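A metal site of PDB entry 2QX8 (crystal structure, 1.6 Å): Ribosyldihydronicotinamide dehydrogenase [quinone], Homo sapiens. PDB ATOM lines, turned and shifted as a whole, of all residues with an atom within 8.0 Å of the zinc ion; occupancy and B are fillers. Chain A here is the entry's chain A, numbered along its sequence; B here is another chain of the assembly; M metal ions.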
ATOM      1  N   TYR A 132      10.777   3.868  -7.455  1.00  0.00           N
ATOM      2  CA  TYR A 132      10.306   4.907  -6.558  1.00  0.00           C
ATOM      3  C   TYR A 132      11.427   5.940  -6.520  1.00  0.00           C
ATOM      4  O   TYR A 132      11.874   6.372  -7.595  1.00  0.00           O
ATOM      5  CB  TYR A 132       9.903   4.359  -5.179  1.00  0.00           C
ATOM      6  CG  TYR A 132       8.524   3.733  -5.244  1.00  0.00           C
ATOM      7  CD1 TYR A 132       7.460   4.423  -5.828  1.00  0.00           C
ATOM      8  CD2 TYR A 132       8.284   2.445  -4.763  1.00  0.00           C
ATOM      9  CE1 TYR A 132       6.200   3.839  -5.952  1.00  0.00           C
ATOM     10  CE2 TYR A 132       7.021   1.838  -4.885  1.00  0.00           C
ATOM     11  CZ  TYR A 132       5.979   2.546  -5.485  1.00  0.00           C
ATOM     12  OH  TYR A 132       4.747   1.951  -5.624  1.00  0.00           O
ATOM     13  N   ASP A 133      11.925   6.340  -5.359  1.00  0.00           N
ATOM     14  CA  ASP A 133      12.991   7.355  -5.350  1.00  0.00           C
ATOM     15  C   ASP A 133      14.228   7.066  -6.199  1.00  0.00           C
ATOM     16  O   ASP A 133      14.883   8.002  -6.700  1.00  0.00           O
ATOM     17  CB  ASP A 133      13.422   7.683  -3.924  1.00  0.00           C
ATOM     18  CG  ASP A 133      12.429   8.550  -3.222  1.00  0.00           C
ATOM     19  OD1 ASP A 133      12.580   8.784  -1.997  1.00  0.00           O
ATOM     20  OD2 ASP A 133      11.478   9.007  -3.900  1.00  0.00           O
ATOM     21  N   TRP A 169      -3.672   8.304  -7.772  1.00  0.00           N
ATOM     22  CA  TRP A 169      -2.729   7.363  -7.198  1.00  0.00           C
ATOM     23  C   TRP A 169      -2.035   6.348  -8.125  1.00  0.00           C
ATOM     24  O   TRP A 169      -0.804   6.272  -8.133  1.00  0.00           O
ATOM     25  CB  TRP A 169      -3.424   6.669  -6.015  1.00  0.00           C
ATOM     26  CG  TRP A 169      -2.627   5.582  -5.381  1.00  0.00           C
ATOM     27  CD1 TRP A 169      -2.848   4.236  -5.475  1.00  0.00           C
ATOM     28  CD2 TRP A 169      -1.561   5.752  -4.445  1.00  0.00           C
ATOM     29  NE1 TRP A 169      -1.999   3.550  -4.639  1.00  0.00           N
ATOM     30  CE2 TRP A 169      -1.194   4.460  -3.983  1.00  0.00           C
ATOM     31  CE3 TRP A 169      -0.896   6.865  -3.933  1.00  0.00           C
ATOM     32  CZ2 TRP A 169      -0.195   4.260  -3.032  1.00  0.00           C
ATOM     33  CZ3 TRP A 169       0.116   6.668  -2.985  1.00  0.00           C
ATOM     34  CH2 TRP A 169       0.449   5.369  -2.546  1.00  0.00           C
ATOM     35  N   LEU A 171      -1.599   6.542 -11.234  1.00  0.00           N
ATOM     36  CA  LEU A 171      -0.810   7.271 -12.235  1.00  0.00           C
ATOM     37  C   LEU A 171       0.391   7.982 -11.634  1.00  0.00           C
ATOM     38  O   LEU A 171       1.505   7.786 -12.081  1.00  0.00           O
ATOM     39  CB  LEU A 171      -1.688   8.284 -12.959  1.00  0.00           C
ATOM     40  CG  LEU A 171      -2.876   7.644 -13.711  1.00  0.00           C
ATOM     41  CD1 LEU A 171      -3.772   8.758 -14.242  1.00  0.00           C
ATOM     42  CD2 LEU A 171      -2.345   6.769 -14.866  1.00  0.00           C
ATOM     43  N   GLN A 172       0.139   8.796 -10.619  1.00  0.00           N
ATOM     44  CA  GLN A 172       1.236   9.554 -10.018  1.00  0.00           C
ATOM     45  C   GLN A 172       2.196   8.729  -9.188  1.00  0.00           C
ATOM     46  O   GLN A 172       3.406   8.862  -9.326  1.00  0.00           O
ATOM     47  CB  GLN A 172       0.684  10.722  -9.192  1.00  0.00           C
ATOM     48  CG  GLN A 172      -0.058  11.735 -10.059  1.00  0.00           C
ATOM     49  CD  GLN A 172      -0.343  13.019  -9.329  1.00  0.00           C
ATOM     50  OE1 GLN A 172      -0.479  14.083  -9.952  1.00  0.00           O
ATOM     51  NE2 GLN A 172      -0.474  12.925  -8.004  1.00  0.00           N
ATOM     52  N   HIS A 173       1.663   7.870  -8.318  1.00  0.00           N
ATOM     53  CA  HIS A 173       2.515   7.047  -7.475  1.00  0.00           C
ATOM     54  C   HIS A 173       2.919   5.714  -8.105  1.00  0.00           C
ATOM     55  O   HIS A 173       4.113   5.385  -8.266  1.00  0.00           O
ATOM     56  CB  HIS A 173       1.799   6.753  -6.155  1.00  0.00           C
ATOM     57  CG  HIS A 173       2.620   5.963  -5.194  1.00  0.00           C
ATOM     58  ND1 HIS A 173       3.589   6.531  -4.391  1.00  0.00           N
ATOM     59  CD2 HIS A 173       2.615   4.647  -4.896  1.00  0.00           C
ATOM     60  CE1 HIS A 173       4.133   5.597  -3.629  1.00  0.00           C
ATOM     61  NE2 HIS A 173       3.556   4.445  -3.912  1.00  0.00           N
ATOM     62  N   GLY A 174       1.909   4.953  -8.489  1.00  0.00           N
ATOM     63  CA  GLY A 174       2.171   3.653  -9.070  1.00  0.00           C
ATOM     64  C   GLY A 174       2.929   3.661 -10.384  1.00  0.00           C
ATOM     65  O   GLY A 174       3.622   2.684 -10.708  1.00  0.00           O
ATOM     66  N   THR A 175       2.807   4.746 -11.155  1.00  0.00           N
ATOM     67  CA  THR A 175       3.534   4.785 -12.422  1.00  0.00           C
ATOM     68  C   THR A 175       4.668   5.812 -12.428  1.00  0.00           C
ATOM     69  O   THR A 175       5.832   5.422 -12.508  1.00  0.00           O
ATOM     70  CB  THR A 175       2.567   5.065 -13.590  1.00  0.00           C
ATOM     71  OG1 THR A 175       1.476   4.133 -13.516  1.00  0.00           O
ATOM     72  CG2 THR A 175       3.241   4.914 -14.938  1.00  0.00           C
ATOM     73  N   LEU A 176       4.354   7.088 -12.317  1.00  0.00           N
ATOM     74  CA  LEU A 176       5.410   8.114 -12.408  1.00  0.00           C
ATOM     75  C   LEU A 176       6.450   8.075 -11.321  1.00  0.00           C
ATOM     76  O   LEU A 176       7.640   7.980 -11.617  1.00  0.00           O
ATOM     77  CB  LEU A 176       4.786   9.512 -12.502  1.00  0.00           C
ATOM     78  CG  LEU A 176       3.843   9.617 -13.727  1.00  0.00           C
ATOM     79  CD1 LEU A 176       3.119  10.950 -13.631  1.00  0.00           C
ATOM     80  CD2 LEU A 176       4.579   9.462 -15.068  1.00  0.00           C
ATOM     81  N   HIS A 177       6.009   8.092 -10.078  1.00  0.00           N
ATOM     82  CA  HIS A 177       6.956   8.037  -8.959  1.00  0.00           C
ATOM     83  C   HIS A 177       7.715   6.717  -8.991  1.00  0.00           C
ATOM     84  O   HIS A 177       8.921   6.656  -8.708  1.00  0.00           O
ATOM     85  CB  HIS A 177       6.217   8.205  -7.628  1.00  0.00           C
ATOM     86  CG  HIS A 177       7.133   8.282  -6.449  1.00  0.00           C
ATOM     87  ND1 HIS A 177       6.672   8.325  -5.151  1.00  0.00           N
ATOM     88  CD2 HIS A 177       8.481   8.343  -6.357  1.00  0.00           C
ATOM     89  CE1 HIS A 177       7.686   8.398  -4.321  1.00  0.00           C
ATOM     90  NE2 HIS A 177       8.803   8.406  -5.026  1.00  0.00           N
ATOM     91  N   PHE A 178       7.039   5.633  -9.338  1.00  0.00           N
ATOM     92  CA  PHE A 178       7.690   4.345  -9.400  1.00  0.00           C
ATOM     93  C   PHE A 178       8.868   4.366 -10.376  1.00  0.00           C
ATOM     94  O   PHE A 178       9.889   3.705 -10.153  1.00  0.00           O
ATOM     95  CB  PHE A 178       6.660   3.250  -9.792  1.00  0.00           C
ATOM     96  CG  PHE A 178       7.212   1.853  -9.755  1.00  0.00           C
ATOM     97  CD1 PHE A 178       7.196   1.110  -8.563  1.00  0.00           C
ATOM     98  CD2 PHE A 178       7.766   1.276 -10.879  1.00  0.00           C
ATOM     99  CE1 PHE A 178       7.741  -0.195  -8.519  1.00  0.00           C
ATOM    100  CE2 PHE A 178       8.310  -0.008 -10.856  1.00  0.00           C
ATOM    101  CZ  PHE A 178       8.307  -0.756  -9.647  1.00  0.00           C
ATOM    102  N   PHE A 181      10.385   9.522 -11.562  1.00  0.00           N
ATOM    103  CA  PHE A 181      10.006  10.901 -11.882  1.00  0.00           C
ATOM    104  C   PHE A 181       9.675  11.719 -10.635  1.00  0.00           C
ATOM    105  O   PHE A 181       9.127  11.204  -9.646  1.00  0.00           O
ATOM    106  CB  PHE A 181       8.712  10.944 -12.729  1.00  0.00           C
ATOM    107  CG  PHE A 181       8.879  10.603 -14.182  1.00  0.00           C
ATOM    108  CD1 PHE A 181       9.457  11.513 -15.075  1.00  0.00           C
ATOM    109  CD2 PHE A 181       8.389   9.399 -14.676  1.00  0.00           C
ATOM    110  CE1 PHE A 181       9.542  11.225 -16.431  1.00  0.00           C
ATOM    111  CE2 PHE A 181       8.467   9.087 -16.050  1.00  0.00           C
ATOM    112  CZ  PHE A 181       9.044  10.026 -16.924  1.00  0.00           C
ATOM    113  N   VAL A 183       7.190  14.281  -9.525  1.00  0.00           N
ATOM    114  CA  VAL A 183       5.893  14.638 -10.050  1.00  0.00           C
ATOM    115  C   VAL A 183       5.415  16.032  -9.735  1.00  0.00           C
ATOM    116  O   VAL A 183       5.211  16.411  -8.573  1.00  0.00           O
ATOM    117  CB  VAL A 183       4.799  13.633  -9.562  1.00  0.00           C
ATOM    118  CG1 VAL A 183       3.423  13.997 -10.142  1.00  0.00           C
ATOM    119  CG2 VAL A 183       5.211  12.212  -9.933  1.00  0.00           C
ATOM    120  N   ILE A 220       5.593  17.532  -6.032  1.00  0.00           N
ATOM    121  CA  ILE A 220       4.732  17.217  -4.884  1.00  0.00           C
ATOM    122  C   ILE A 220       5.361  16.054  -4.107  1.00  0.00           C
ATOM    123  O   ILE A 220       6.257  15.381  -4.605  1.00  0.00           O
ATOM    124  CB  ILE A 220       3.317  16.751  -5.308  1.00  0.00           C
ATOM    125  CG1 ILE A 220       3.433  15.438  -6.092  1.00  0.00           C
ATOM    126  CG2 ILE A 220       2.633  17.832  -6.130  1.00  0.00           C
ATOM    127  CD1 ILE A 220       2.113  14.719  -6.288  1.00  0.00           C
ATOM    128  N   PRO A 221       4.932  15.843  -2.854  1.00  0.00           N
ATOM    129  CA  PRO A 221       5.522  14.708  -2.132  1.00  0.00           C
ATOM    130  C   PRO A 221       4.615  13.555  -2.578  1.00  0.00           C
ATOM    131  O   PRO A 221       3.439  13.517  -2.217  1.00  0.00           O
ATOM    132  CB  PRO A 221       5.322  15.086  -0.664  1.00  0.00           C
ATOM    133  CG  PRO A 221       4.029  15.875  -0.691  1.00  0.00           C
ATOM    134  CD  PRO A 221       4.158  16.723  -1.954  1.00  0.00           C
ATOM    135  N   CYS A 222       5.141  12.656  -3.382  1.00  0.00           N
ATOM    136  CA  CYS A 222       4.300  11.570  -3.878  1.00  0.00           C
ATOM    137  C   CYS A 222       4.134  10.454  -2.848  1.00  0.00           C
ATOM    138  O   CYS A 222       4.796   9.419  -2.895  1.00  0.00           O
ATOM    139  CB  CYS A 222       4.870  11.043  -5.183  1.00  0.00           C
ATOM    140  SG  CYS A 222       3.586  10.239  -6.160  1.00  0.00           S
ATOM    141  N   THR A 223       3.212  10.677  -1.921  1.00  0.00           N
ATOM    142  CA  THR A 223       2.953   9.746  -0.840  1.00  0.00           C
ATOM    143  C   THR A 223       1.480   9.395  -0.725  1.00  0.00           C
ATOM    144  O   THR A 223       0.629  10.050  -1.302  1.00  0.00           O
ATOM    145  CB  THR A 223       3.351  10.376   0.505  1.00  0.00           C
ATOM    146  OG1 THR A 223       2.516  11.521   0.748  1.00  0.00           O
ATOM    147  CG2 THR A 223       4.797  10.825   0.472  1.00  0.00           C
ATOM    148  N   ALA A 224       1.193   8.376   0.070  1.00  0.00           N
ATOM    149  CA  ALA A 224      -0.186   7.971   0.300  1.00  0.00           C
ATOM    150  C   ALA A 224      -0.885   9.118   1.016  1.00  0.00           C
ATOM    151  O   ALA A 224      -2.059   9.394   0.806  1.00  0.00           O
ATOM    152  CB  ALA A 224      -0.213   6.710   1.154  1.00  0.00           C
ATOM    153  N   TRP A 226      -0.324  12.453   0.712  1.00  0.00           N
ATOM    154  CA  TRP A 226      -0.705  13.513  -0.216  1.00  0.00           C
ATOM    155  C   TRP A 226      -2.010  13.147  -0.926  1.00  0.00           C
ATOM    156  O   TRP A 226      -2.904  13.981  -1.074  1.00  0.00           O
ATOM    157  CB  TRP A 226       0.383  13.725  -1.285  1.00  0.00           C
ATOM    158  CG  TRP A 226       0.104  14.895  -2.231  1.00  0.00           C
ATOM    159  CD1 TRP A 226       0.508  16.187  -2.082  1.00  0.00           C
ATOM    160  CD2 TRP A 226      -0.682  14.869  -3.442  1.00  0.00           C
ATOM    161  NE1 TRP A 226       0.041  16.965  -3.109  1.00  0.00           N
ATOM    162  CE2 TRP A 226      -0.696  16.178  -3.961  1.00  0.00           C
ATOM    163  CE3 TRP A 226      -1.370  13.856  -4.148  1.00  0.00           C
ATOM    164  CZ2 TRP A 226      -1.375  16.515  -5.143  1.00  0.00           C
ATOM    165  CZ3 TRP A 226      -2.046  14.193  -5.321  1.00  0.00           C
ATOM    166  CH2 TRP A 226      -2.043  15.520  -5.814  1.00  0.00           C
ATOM    167  N   HIS A 227      -2.131  11.885  -1.354  1.00  0.00           N
ATOM    168  CA  HIS A 227      -3.321  11.424  -2.083  1.00  0.00           C
ATOM    169  C   HIS A 227      -4.586  11.185  -1.261  1.00  0.00           C
ATOM    170  O   HIS A 227      -5.691  11.598  -1.648  1.00  0.00           O
ATOM    171  CB  HIS A 227      -3.020  10.142  -2.869  1.00  0.00           C
ATOM    172  CG  HIS A 227      -2.088  10.333  -4.025  1.00  0.00           C
ATOM    173  ND1 HIS A 227      -0.714  10.349  -3.885  1.00  0.00           N
ATOM    174  CD2 HIS A 227      -2.330  10.513  -5.346  1.00  0.00           C
ATOM    175  CE1 HIS A 227      -0.158  10.547  -5.073  1.00  0.00           C
ATOM    176  NE2 HIS A 227      -1.122  10.646  -5.975  1.00  0.00           N
ATOM    177  N   VAL B 160       5.640  -0.053   0.409  1.00  0.00           N
ATOM    178  CA  VAL B 160       5.959   0.946  -0.617  1.00  0.00           C
ATOM    179  C   VAL B 160       4.848   1.226  -1.610  1.00  0.00           C
ATOM    180  O   VAL B 160       4.667   2.364  -2.083  1.00  0.00           O
ATOM    181  CB  VAL B 160       7.250   0.544  -1.410  1.00  0.00           C
ATOM    182  CG1 VAL B 160       8.486   0.814  -0.557  1.00  0.00           C
ATOM    183  CG2 VAL B 160       7.193  -0.929  -1.809  1.00  0.00           C
HETATM  184 ZN    ZN M   1       4.523   8.447  -4.945  1.00  0.00          ZN
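The zinc ion is bound by a ring nitrogen (ND1) of His 177 (2.2 Å), a ring nitrogen (ND1) of His 173 (2.2 Å), the backbone carbonyl oxygen (O) of Cys 222 (2.3 Å) and the side-chain sulfur (SG) of Cys 222 (2.4 Å).
The backbone NH of His 177 sits at hydrogen-bond distance from the backbone carbonyl oxygen of Gln 172 (2.8 Å).
NE2 of His 177 lies within hydrogen-bond range of OD2 of Asp 133 (3.0 Å).
OH of Tyr 132 is in hydrogen-bond range of NE2 of His 173 (3.3 Å).
The backbone carbonyl oxygen (O) of His 173 sits at hydrogen-bond distance from the backbone NH (N) of Phe 178 (3.1 Å).
NE2 of His 173 is in hydrogen-bond range of O of Val 160 of chain B (3.0 Å).
SG of Cys 222 sits close to O of Gln 172.
ND1 of His 227 is in hydrogen-bond range of O of Thr 223.
The backbone NH (N) of Trp 226 lies within hydrogen-bond range of the side-chain hydroxyl (OG1) of Thr 223 (3.0 Å).
N of Thr 223 touches the zinc ion, at 3.98 Å.
Within 4 Å of the zinc ion: His 173, His 177, Cys 222 and Thr 223.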
